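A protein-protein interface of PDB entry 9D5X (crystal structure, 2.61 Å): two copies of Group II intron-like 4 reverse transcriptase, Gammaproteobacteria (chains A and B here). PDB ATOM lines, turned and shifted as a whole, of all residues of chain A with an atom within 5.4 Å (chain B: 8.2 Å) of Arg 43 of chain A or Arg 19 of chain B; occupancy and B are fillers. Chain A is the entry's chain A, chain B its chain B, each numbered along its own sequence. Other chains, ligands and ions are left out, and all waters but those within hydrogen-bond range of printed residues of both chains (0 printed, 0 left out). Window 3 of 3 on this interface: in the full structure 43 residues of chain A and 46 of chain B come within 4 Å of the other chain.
The backbone carbonyl oxygen of Ser 42 of chain A lies within hydrogen-bond range of the guanidinium group of Arg 19 of chain B (2.5 Å).
OE2 of Glu 41 of chain A sits close to OE2 of Glu 41 of chain B, at 3.2 Å.
O of Arg 43 of chain A is in hydrogen-bond range of OG of Ser 47 of chain A (2.8 Å).
NH2 of Arg 43 of chain A is in salt-bridge range of OE1 of Glu 50 of chain A, 3.3 Å away.
O of Leu 44 of chain A is in hydrogen-bond range of OG of Ser 47 of chain A, 3.3 Å away.
OG of Ser 23 of chain B is in hydrogen-bond range of O of Arg 19 of chain B (3.1 Å).
The side-chain carboxylate (OE2) of Glu 41 of chain B is in salt-bridge range of the guanidinium group (NH1) of Arg 22 of chain B, 2.9 Å away.
Among the printed residues, merely in contact across the chains: Leu 44 of chain A with Tyr 15 of chain B, Pro 45 of chain A with Arg 19 of chain B, Leu 44 of chain A with Arg 22 of chain B, Pro 45 of chain A with Tyr 15 of chain B, Glu 41 of chain A with Arg 19 of chain B, Arg 43 of chain A with Arg 19 of chain B, Leu 44 of chain A with Arg 19 of chain B and Leu 44 of chain A with Glu 41 of chain B.
Arg 19 of chain B touches just these residues of chain A: Glu 41 (3.6 Å), Ser 42 (2.5 Å), Arg 43 (3.8 Å), Leu 44 (3.8 Å) and Pro 45 (3.4 Å).
Printed residues of chain B within 4 Å of Ser 42 of chain A: Arg 19.
Printed residues of chain A within 4 Å of Tyr 15 of chain B: Leu 44 and Pro 45.
Of the printed residues of chain B, Glu 41 of chain A touches Arg 19 (3.6 Å) and Glu 41 (3.2 Å).
Printed residues of chain A within 4 Å of Arg 22 of chain B: Leu 44 (3.5 Å).
Of the printed residues of chain B, Leu 44 of chain A touches Tyr 15 (3.2 Å), Arg 19 (3.8 Å), Arg 22 (3.5 Å) and Glu 41 (3.8 Å).
Asp 46 of chain A touches none of the printed residues of chain B.
The nearest residue of chain B that does not touch Arg 43 of chain A is Tyr 15 of chain B (6.2 Å).
The nearest printed residue of chain A that does not touch Arg 22 of chain B is Glu 41 of chain A (4.03 Å).
Of the 20 printed residues of chain B, 4 touch a printed residue of chain A.
Of the 11 printed residues of chain A, 5 touch a printed residue of chain B.
Among the printed residues, 10 pairs touch across the chains.
Glu 41 of chain A touches its own counterpart, Glu 41 of chain B.
Leu 44 of chain A touches Glu 41 of chain B, but with the chains exchanged Glu 41 of chain A does not touch Leu 44 of chain B (6.6 Å).
Positions printed for both chains: 41, 44 and 48.
Of the 10 pairs that touch across the chains among the printed residues, 1 has its exchanged pair printed and touching as well.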
ATOM      1  N   GLU A  39      28.144  -9.259  17.532  1.00  0.00           N
ATOM      2  CA  GLU A  39      28.134  -7.819  17.295  1.00  0.00           C
ATOM      3  C   GLU A  39      26.747  -7.234  17.537  1.00  0.00           C
ATOM      4  O   GLU A  39      26.617  -6.138  18.094  1.00  0.00           O
ATOM      5  CB  GLU A  39      28.617  -7.515  15.877  1.00  0.00           C
ATOM      6  CG  GLU A  39      29.115  -6.089  15.682  1.00  0.00           C
ATOM      7  CD  GLU A  39      28.007  -5.117  15.332  1.00  0.00           C
ATOM      8  OE1 GLU A  39      27.518  -5.158  14.184  1.00  0.00           O
ATOM      9  OE2 GLU A  39      27.621  -4.312  16.207  1.00  0.00           O
ATOM     10  N   PHE A  40      25.697  -7.950  17.126  1.00  0.00           N
ATOM     11  CA  PHE A  40      24.343  -7.535  17.476  1.00  0.00           C
ATOM     12  C   PHE A  40      24.106  -7.652  18.977  1.00  0.00           C
ATOM     13  O   PHE A  40      23.315  -6.887  19.543  1.00  0.00           O
ATOM     14  CB  PHE A  40      23.320  -8.368  16.702  1.00  0.00           C
ATOM     15  CG  PHE A  40      21.906  -7.870  16.828  1.00  0.00           C
ATOM     16  CD1 PHE A  40      21.424  -6.889  15.978  1.00  0.00           C
ATOM     17  CD2 PHE A  40      21.056  -8.389  17.790  1.00  0.00           C
ATOM     18  CE1 PHE A  40      20.124  -6.431  16.090  1.00  0.00           C
ATOM     19  CE2 PHE A  40      19.756  -7.937  17.907  1.00  0.00           C
ATOM     20  CZ  PHE A  40      19.289  -6.955  17.056  1.00  0.00           C
ATOM     21  N   GLU A  41      24.785  -8.595  19.633  1.00  0.00           N
ATOM     22  CA  GLU A  41      24.694  -8.729  21.081  1.00  0.00           C
ATOM     23  C   GLU A  41      25.428  -7.610  21.809  1.00  0.00           C
ATOM     24  O   GLU A  41      25.110  -7.326  22.968  1.00  0.00           O
ATOM     25  CB  GLU A  41      25.246 -10.092  21.504  1.00  0.00           C
ATOM     26  CG  GLU A  41      24.884 -10.519  22.915  1.00  0.00           C
ATOM     27  CD  GLU A  41      25.347 -11.927  23.229  1.00  0.00           C
ATOM     28  OE1 GLU A  41      26.204 -12.452  22.488  1.00  0.00           O
ATOM     29  OE2 GLU A  41      24.851 -12.511  24.215  1.00  0.00           O
ATOM     30  N   SER A  42      26.398  -6.964  21.151  1.00  0.00           N
ATOM     31  CA  SER A  42      27.138  -5.870  21.770  1.00  0.00           C
ATOM     32  C   SER A  42      26.281  -4.626  21.955  1.00  0.00           C
ATOM     33  O   SER A  42      26.657  -3.738  22.727  1.00  0.00           O
ATOM     34  CB  SER A  42      28.369  -5.523  20.933  1.00  0.00           C
ATOM     35  OG  SER A  42      29.268  -6.617  20.864  1.00  0.00           O
ATOM     36  N   ARG A  43      25.142  -4.542  21.270  1.00  0.00           N
ATOM     37  CA  ARG A  43      24.200  -3.439  21.424  1.00  0.00           C
ATOM     38  C   ARG A  43      22.838  -3.946  21.890  1.00  0.00           C
ATOM     39  O   ARG A  43      21.807  -3.328  21.611  1.00  0.00           O
ATOM     40  CB  ARG A  43      24.065  -2.666  20.113  1.00  0.00           C
ATOM     41  CG  ARG A  43      23.583  -1.228  20.260  1.00  0.00           C
ATOM     42  CD  ARG A  43      23.511  -0.532  18.908  1.00  0.00           C
ATOM     43  NE  ARG A  43      22.888  -1.378  17.898  1.00  0.00           N
ATOM     44  CZ  ARG A  43      22.543  -0.967  16.685  1.00  0.00           C
ATOM     45  NH1 ARG A  43      22.723   0.287  16.302  1.00  0.00           N
ATOM     46  NH2 ARG A  43      22.002  -1.836  15.836  1.00  0.00           N
ATOM     47  N   LEU A  44      22.835  -5.061  22.630  1.00  0.00           N
ATOM     48  CA  LEU A  44      21.619  -5.783  23.030  1.00  0.00           C
ATOM     49  C   LEU A  44      20.448  -4.902  23.457  1.00  0.00           C
ATOM     50  O   LEU A  44      19.326  -5.169  23.006  1.00  0.00           O
ATOM     51  CB  LEU A  44      21.971  -6.779  24.146  1.00  0.00           C
ATOM     52  CG  LEU A  44      21.982  -8.263  23.761  1.00  0.00           C
ATOM     53  CD1 LEU A  44      22.258  -9.091  24.992  1.00  0.00           C
ATOM     54  CD2 LEU A  44      20.659  -8.654  23.125  1.00  0.00           C
ATOM     55  N   PRO A  45      20.613  -3.852  24.295  1.00  0.00           N
ATOM     56  CA  PRO A  45      19.450  -3.025  24.643  1.00  0.00           C
ATOM     57  C   PRO A  45      18.851  -2.313  23.442  1.00  0.00           C
ATOM     58  O   PRO A  45      17.688  -2.540  23.103  1.00  0.00           O
ATOM     59  CB  PRO A  45      20.016  -2.028  25.665  1.00  0.00           C
ATOM     60  CG  PRO A  45      21.479  -2.024  25.453  1.00  0.00           C
ATOM     61  CD  PRO A  45      21.805  -3.435  25.054  1.00  0.00           C
ATOM     62  N   ASP A  46      19.640  -1.459  22.791  1.00  0.00           N
ATOM     63  CA  ASP A  46      19.118  -0.623  21.718  1.00  0.00           C
ATOM     64  C   ASP A  46      19.014  -1.353  20.384  1.00  0.00           C
ATOM     65  O   ASP A  46      18.314  -0.869  19.489  1.00  0.00           O
ATOM     66  CB  ASP A  46      19.991   0.623  21.559  1.00  0.00           C
ATOM     67  CG  ASP A  46      20.087   1.432  22.839  1.00  0.00           C
ATOM     68  OD1 ASP A  46      20.809   1.002  23.764  1.00  0.00           O
ATOM     69  OD2 ASP A  46      19.438   2.496  22.922  1.00  0.00           O
ATOM     70  N   SER A  47      19.684  -2.495  20.224  1.00  0.00           N
ATOM     71  CA  SER A  47      19.624  -3.209  18.952  1.00  0.00           C
ATOM     72  C   SER A  47      18.240  -3.804  18.721  1.00  0.00           C
ATOM     73  O   SER A  47      17.664  -3.661  17.636  1.00  0.00           O
ATOM     74  CB  SER A  47      20.696  -4.298  18.902  1.00  0.00           C
ATOM     75  OG  SER A  47      20.515  -5.242  19.943  1.00  0.00           O
ATOM     76  N   LEU A  48      17.688  -4.480  19.731  1.00  0.00           N
ATOM     77  CA  LEU A  48      16.343  -5.025  19.615  1.00  0.00           C
ATOM     78  C   LEU A  48      15.264  -3.970  19.812  1.00  0.00           C
ATOM     79  O   LEU A  48      14.138  -4.158  19.338  1.00  0.00           O
ATOM     80  CB  LEU A  48      16.142  -6.161  20.619  1.00  0.00           C
ATOM     81  CG  LEU A  48      16.807  -7.493  20.266  1.00  0.00           C
ATOM     82  CD1 LEU A  48      16.541  -8.531  21.345  1.00  0.00           C
ATOM     83  CD2 LEU A  48      16.318  -7.988  18.912  1.00  0.00           C
ATOM     84  N   GLU A  50      15.530  -0.818  18.625  1.00  0.00           N
ATOM     85  CA  GLU A  50      15.430  -0.184  17.313  1.00  0.00           C
ATOM     86  C   GLU A  50      14.451  -0.928  16.414  1.00  0.00           C
ATOM     87  O   GLU A  50      13.675  -0.309  15.678  1.00  0.00           O
ATOM     88  CB  GLU A  50      16.806  -0.113  16.650  1.00  0.00           C
ATOM     89  CG  GLU A  50      17.655   1.075  17.069  1.00  0.00           C
ATOM     90  CD  GLU A  50      19.010   1.081  16.389  1.00  0.00           C
ATOM     91  OE1 GLU A  50      19.340   0.080  15.718  1.00  0.00           O
ATOM     92  OE2 GLU A  50      19.742   2.084  16.522  1.00  0.00           O
ATOM     93  N   ARG B  12      15.204   1.300  30.794  1.00  0.00           N
ATOM     94  CA  ARG B  12      16.389   1.853  30.144  1.00  0.00           C
ATOM     95  C   ARG B  12      17.590   1.823  31.081  1.00  0.00           C
ATOM     96  O   ARG B  12      18.665   1.337  30.715  1.00  0.00           O
ATOM     97  CB  ARG B  12      16.111   3.281  29.670  1.00  0.00           C
ATOM     98  CG  ARG B  12      17.297   3.939  28.982  1.00  0.00           C
ATOM     99  CD  ARG B  12      17.053   5.419  28.709  1.00  0.00           C
ATOM    100  NE  ARG B  12      15.899   5.649  27.847  1.00  0.00           N
ATOM    101  CZ  ARG B  12      14.741   6.149  28.260  1.00  0.00           C
ATOM    102  NH1 ARG B  12      14.548   6.498  29.522  1.00  0.00           N
ATOM    103  NH2 ARG B  12      13.754   6.308  27.382  1.00  0.00           N
ATOM    104  N   THR B  13      17.421   2.337  32.302  1.00  0.00           N
ATOM    105  CA  THR B  13      18.531   2.353  33.248  1.00  0.00           C
ATOM    106  C   THR B  13      18.781   0.976  33.850  1.00  0.00           C
ATOM    107  O   THR B  13      19.929   0.642  34.166  1.00  0.00           O
ATOM    108  CB  THR B  13      18.264   3.374  34.355  1.00  0.00           C
ATOM    109  OG1 THR B  13      17.168   2.931  35.167  1.00  0.00           O
ATOM    110  CG2 THR B  13      17.922   4.722  33.749  1.00  0.00           C
ATOM    111  N   LEU B  14      17.729   0.170  34.020  1.00  0.00           N
ATOM    112  CA  LEU B  14      17.910  -1.182  34.542  1.00  0.00           C
ATOM    113  C   LEU B  14      18.693  -2.045  33.558  1.00  0.00           C
ATOM    114  O   LEU B  14      19.696  -2.670  33.925  1.00  0.00           O
ATOM    115  CB  LEU B  14      16.552  -1.810  34.855  1.00  0.00           C
ATOM    116  CG  LEU B  14      15.783  -1.207  36.030  1.00  0.00           C
ATOM    117  CD1 LEU B  14      14.457  -1.915  36.209  1.00  0.00           C
ATOM    118  CD2 LEU B  14      16.607  -1.285  37.307  1.00  0.00           C
ATOM    119  N   TYR B  15      18.247  -2.093  32.300  1.00  0.00           N
ATOM    120  CA  TYR B  15      19.009  -2.799  31.275  1.00  0.00           C
ATOM    121  C   TYR B  15      20.392  -2.183  31.111  1.00  0.00           C
ATOM    122  O   TYR B  15      21.384  -2.901  30.926  1.00  0.00           O
ATOM    123  CB  TYR B  15      18.238  -2.785  29.952  1.00  0.00           C
ATOM    124  CG  TYR B  15      18.609  -3.887  28.977  1.00  0.00           C
ATOM    125  CD1 TYR B  15      19.926  -4.095  28.594  1.00  0.00           C
ATOM    126  CD2 TYR B  15      17.634  -4.716  28.438  1.00  0.00           C
ATOM    127  CE1 TYR B  15      20.267  -5.093  27.707  1.00  0.00           C
ATOM    128  CE2 TYR B  15      17.964  -5.717  27.547  1.00  0.00           C
ATOM    129  CZ  TYR B  15      19.283  -5.901  27.185  1.00  0.00           C
ATOM    130  OH  TYR B  15      19.623  -6.897  26.301  1.00  0.00           O
ATOM    131  N   GLY B  16      20.481  -0.853  31.193  1.00  0.00           N
ATOM    132  CA  GLY B  16      21.781  -0.206  31.141  1.00  0.00           C
ATOM    133  C   GLY B  16      22.693  -0.620  32.278  1.00  0.00           C
ATOM    134  O   GLY B  16      23.915  -0.686  32.107  1.00  0.00           O
ATOM    135  N   ALA B  17      22.122  -0.912  33.447  1.00  0.00           N
ATOM    136  CA  ALA B  17      22.926  -1.362  34.578  1.00  0.00           C
ATOM    137  C   ALA B  17      23.338  -2.819  34.443  1.00  0.00           C
ATOM    138  O   ALA B  17      24.397  -3.207  34.952  1.00  0.00           O
ATOM    139  CB  ALA B  17      22.161  -1.158  35.887  1.00  0.00           C
ATOM    140  N   TRP B  18      22.527  -3.638  33.768  1.00  0.00           N
ATOM    141  CA  TRP B  18      22.849  -5.056  33.646  1.00  0.00           C
ATOM    142  C   TRP B  18      24.133  -5.276  32.858  1.00  0.00           C
ATOM    143  O   TRP B  18      24.888  -6.210  33.149  1.00  0.00           O
ATOM    144  CB  TRP B  18      21.695  -5.810  32.986  1.00  0.00           C
ATOM    145  CG  TRP B  18      21.593  -7.218  33.465  1.00  0.00           C
ATOM    146  CD1 TRP B  18      20.816  -7.675  34.484  1.00  0.00           C
ATOM    147  CD2 TRP B  18      22.306  -8.353  32.963  1.00  0.00           C
ATOM    148  NE1 TRP B  18      21.000  -9.022  34.650  1.00  0.00           N
ATOM    149  CE2 TRP B  18      21.905  -9.466  33.726  1.00  0.00           C
ATOM    150  CE3 TRP B  18      23.240  -8.539  31.942  1.00  0.00           C
ATOM    151  CZ2 TRP B  18      22.405 -10.745  33.498  1.00  0.00           C
ATOM    152  CZ3 TRP B  18      23.735  -9.810  31.721  1.00  0.00           C
ATOM    153  CH2 TRP B  18      23.317 -10.895  32.493  1.00  0.00           C
ATOM    154  N   ARG B  19      24.401  -4.425  31.866  1.00  0.00           N
ATOM    155  CA  ARG B  19      25.605  -4.587  31.060  1.00  0.00           C
ATOM    156  C   ARG B  19      26.860  -4.351  31.889  1.00  0.00           C
ATOM    157  O   ARG B  19      27.856  -5.068  31.737  1.00  0.00           O
ATOM    158  CB  ARG B  19      25.562  -3.633  29.867  1.00  0.00           C
ATOM    159  CG  ARG B  19      24.165  -3.410  29.315  1.00  0.00           C
ATOM    160  CD  ARG B  19      24.223  -2.821  27.923  1.00  0.00           C
ATOM    161  NE  ARG B  19      24.847  -3.749  26.987  1.00  0.00           N
ATOM    162  CZ  ARG B  19      25.168  -3.450  25.737  1.00  0.00           C
ATOM    163  NH1 ARG B  19      24.947  -2.247  25.234  1.00  0.00           N
ATOM    164  NH2 ARG B  19      25.726  -4.384  24.971  1.00  0.00           N
ATOM    165  N   LYS B  20      26.830  -3.351  32.775  1.00  0.00           N
ATOM    166  CA  LYS B  20      27.968  -3.104  33.652  1.00  0.00           C
ATOM    167  C   LYS B  20      28.181  -4.262  34.618  1.00  0.00           C
ATOM    168  O   LYS B  20      29.324  -4.643  34.899  1.00  0.00           O
ATOM    169  CB  LYS B  20      27.765  -1.795  34.414  1.00  0.00           C
ATOM    170  CG  LYS B  20      27.773  -0.559  33.528  1.00  0.00           C
ATOM    171  CD  LYS B  20      26.610   0.364  33.852  1.00  0.00           C
ATOM    172  CE  LYS B  20      26.697   1.659  33.061  1.00  0.00           C
ATOM    173  NZ  LYS B  20      25.505   2.526  33.277  1.00  0.00           N
ATOM    174  N   VAL B  21      27.091  -4.832  35.137  1.00  0.00           N
ATOM    175  CA  VAL B  21      27.201  -6.002  36.005  1.00  0.00           C
ATOM    176  C   VAL B  21      27.773  -7.183  35.229  1.00  0.00           C
ATOM    177  O   VAL B  21      28.555  -7.980  35.764  1.00  0.00           O
ATOM    178  CB  VAL B  21      25.830  -6.339  36.620  1.00  0.00           C
ATOM    179  CG1 VAL B  21      25.922  -7.579  37.493  1.00  0.00           C
ATOM    180  CG2 VAL B  21      25.302  -5.156  37.419  1.00  0.00           C
ATOM    181  N   ARG B  22      27.399  -7.306  33.953  1.00  0.00           N
ATOM    182  CA  ARG B  22      27.917  -8.387  33.120  1.00  0.00           C
ATOM    183  C   ARG B  22      29.420  -8.255  32.907  1.00  0.00           C
ATOM    184  O   ARG B  22      30.154  -9.244  32.999  1.00  0.00           O
ATOM    185  CB  ARG B  22      27.185  -8.405  31.778  1.00  0.00           C
ATOM    186  CG  ARG B  22      27.840  -9.272  30.721  1.00  0.00           C
ATOM    187  CD  ARG B  22      26.834 -10.221  30.093  1.00  0.00           C
ATOM    188  NE  ARG B  22      25.718  -9.511  29.478  1.00  0.00           N
ATOM    189  CZ  ARG B  22      25.406  -9.566  28.193  1.00  0.00           C
ATOM    190  NH1 ARG B  22      26.106 -10.297  27.342  1.00  0.00           N
ATOM    191  NH2 ARG B  22      24.359  -8.875  27.751  1.00  0.00           N
ATOM    192  N   SER B  23      29.893  -7.039  32.620  1.00  0.00           N
ATOM    193  CA  SER B  23      31.318  -6.839  32.370  1.00  0.00           C
ATOM    194  C   SER B  23      32.139  -7.099  33.626  1.00  0.00           C
ATOM    195  O   SER B  23      33.167  -7.783  33.576  1.00  0.00           O
ATOM    196  CB  SER B  23      31.561  -5.421  31.851  1.00  0.00           C
ATOM    197  OG  SER B  23      30.788  -5.162  30.694  1.00  0.00           O
ATOM    198  N   SER B  24      31.693  -6.561  34.765  1.00  0.00           N
ATOM    199  CA  SER B  24      32.402  -6.770  36.024  1.00  0.00           C
ATOM    200  C   SER B  24      32.537  -8.249  36.358  1.00  0.00           C
ATOM    201  O   SER B  24      33.519  -8.658  36.989  1.00  0.00           O
ATOM    202  CB  SER B  24      31.681  -6.037  37.154  1.00  0.00           C
ATOM    203  OG  SER B  24      31.676  -4.636  36.936  1.00  0.00           O
ATOM    204  N   ALA B  25      31.567  -9.065  35.942  1.00  0.00           N
ATOM    205  CA  ALA B  25      31.642 -10.504  36.164  1.00  0.00           C
ATOM    206  C   ALA B  25      32.619 -11.170  35.201  1.00  0.00           C
ATOM    207  O   ALA B  25      33.420 -12.016  35.613  1.00  0.00           O
ATOM    208  CB  ALA B  25      30.253 -11.125  36.027  1.00  0.00           C
ATOM    209  N   PHE B  26      32.571 -10.797  33.918  1.00  0.00           N
ATOM    210  CA  PHE B  26      33.468 -11.406  32.939  1.00  0.00           C
ATOM    211  C   PHE B  26      34.922 -11.028  33.191  1.00  0.00           C
ATOM    212  O   PHE B  26      35.828 -11.780  32.815  1.00  0.00           O
ATOM    213  CB  PHE B  26      33.052 -11.008  31.524  1.00  0.00           C
ATOM    214  CG  PHE B  26      31.870 -11.772  31.003  1.00  0.00           C
ATOM    215  CD1 PHE B  26      31.651 -13.082  31.395  1.00  0.00           C
ATOM    216  CD2 PHE B  26      30.980 -11.185  30.122  1.00  0.00           C
ATOM    217  CE1 PHE B  26      30.566 -13.791  30.918  1.00  0.00           C
ATOM    218  CE2 PHE B  26      29.893 -11.890  29.642  1.00  0.00           C
ATOM    219  CZ  PHE B  26      29.686 -13.194  30.042  1.00  0.00           C
ATOM    220  N   GLU B  41      20.748 -13.986  31.927  1.00  0.00           N
ATOM    221  CA  GLU B  41      20.625 -13.574  30.535  1.00  0.00           C
ATOM    222  C   GLU B  41      19.687 -14.490  29.757  1.00  0.00           C
ATOM    223  O   GLU B  41      19.042 -14.045  28.802  1.00  0.00           O
ATOM    224  CB  GLU B  41      22.008 -13.544  29.886  1.00  0.00           C
ATOM    225  CG  GLU B  41      22.047 -12.934  28.499  1.00  0.00           C
ATOM    226  CD  GLU B  41      23.455 -12.837  27.946  1.00  0.00           C
ATOM    227  OE1 GLU B  41      24.311 -13.654  28.346  1.00  0.00           O
ATOM    228  OE2 GLU B  41      23.705 -11.938  27.116  1.00  0.00           O
ATOM    229  N   LEU B  44      16.296 -12.954  29.801  1.00  0.00           N
ATOM    230  CA  LEU B  44      16.481 -11.503  29.763  1.00  0.00           C
ATOM    231  C   LEU B  44      15.195 -10.679  29.736  1.00  0.00           C
ATOM    232  O   LEU B  44      15.128  -9.684  30.478  1.00  0.00           O
ATOM    233  CB  LEU B  44      17.367 -11.135  28.564  1.00  0.00           C
ATOM    234  CG  LEU B  44      18.811 -10.761  28.904  1.00  0.00           C
ATOM    235  CD1 LEU B  44      19.610 -10.499  27.642  1.00  0.00           C
ATOM    236  CD2 LEU B  44      18.846  -9.548  29.823  1.00  0.00           C
ATOM    237  N   LEU B  48      14.439  -8.974  33.985  1.00  0.00           N
ATOM    238  CA  LEU B  48      14.566  -7.573  34.370  1.00  0.00           C
ATOM    239  C   LEU B  48      13.222  -6.900  34.603  1.00  0.00           C
ATOM    240  O   LEU B  48      13.145  -5.944  35.381  1.00  0.00           O
ATOM    241  CB  LEU B  48      15.345  -6.793  33.311  1.00  0.00           C
ATOM    242  CG  LEU B  48      16.849  -6.673  33.561  1.00  0.00           C
ATOM    243  CD1 LEU B  48      17.539  -5.959  32.411  1.00  0.00           C
ATOM    244  CD2 LEU B  48      17.110  -5.951  34.876  1.00  0.00           C
ATOM    245  N   VAL B  89      22.367  -5.471  40.136  1.00  0.00           N
ATOM    246  CA  VAL B  89      21.851  -4.572  39.109  1.00  0.00           C
ATOM    247  C   VAL B  89      21.184  -3.360  39.742  1.00  0.00           C
ATOM    248  O   VAL B  89      21.360  -2.225  39.280  1.00  0.00           O
ATOM    249  CB  VAL B  89      20.891  -5.328  38.174  1.00  0.00           C
ATOM    250  CG1 VAL B  89      20.227  -4.369  37.195  1.00  0.00           C
ATOM    251  CG2 VAL B  89      21.640  -6.414  37.429  1.00  0.00           C
ATOM    252  N   ARG B  92      23.790  -0.967  40.791  1.00  0.00           N
ATOM    253  CA  ARG B  92      24.359  -0.250  39.654  1.00  0.00           C
ATOM    254  C   ARG B  92      23.368   0.759  39.086  1.00  0.00           C
ATOM    255  O   ARG B  92      23.758   1.862  38.683  1.00  0.00           O
ATOM    256  CB  ARG B  92      24.796  -1.238  38.573  1.00  0.00           C
ATOM    257  CG  ARG B  92      25.529  -0.586  37.415  1.00  0.00           C
ATOM    258  CD  ARG B  92      26.882  -0.060  37.859  1.00  0.00           C
ATOM    259  NE  ARG B  92      27.318   1.072  37.053  1.00  0.00           N
ATOM    260  CZ  ARG B  92      28.512   1.641  37.147  1.00  0.00           C
ATOM    261  NH1 ARG B  92      29.429   1.190  37.986  1.00  0.00           N
ATOM    262  NH2 ARG B  92      28.793   2.688  36.377  1.00  0.00           N
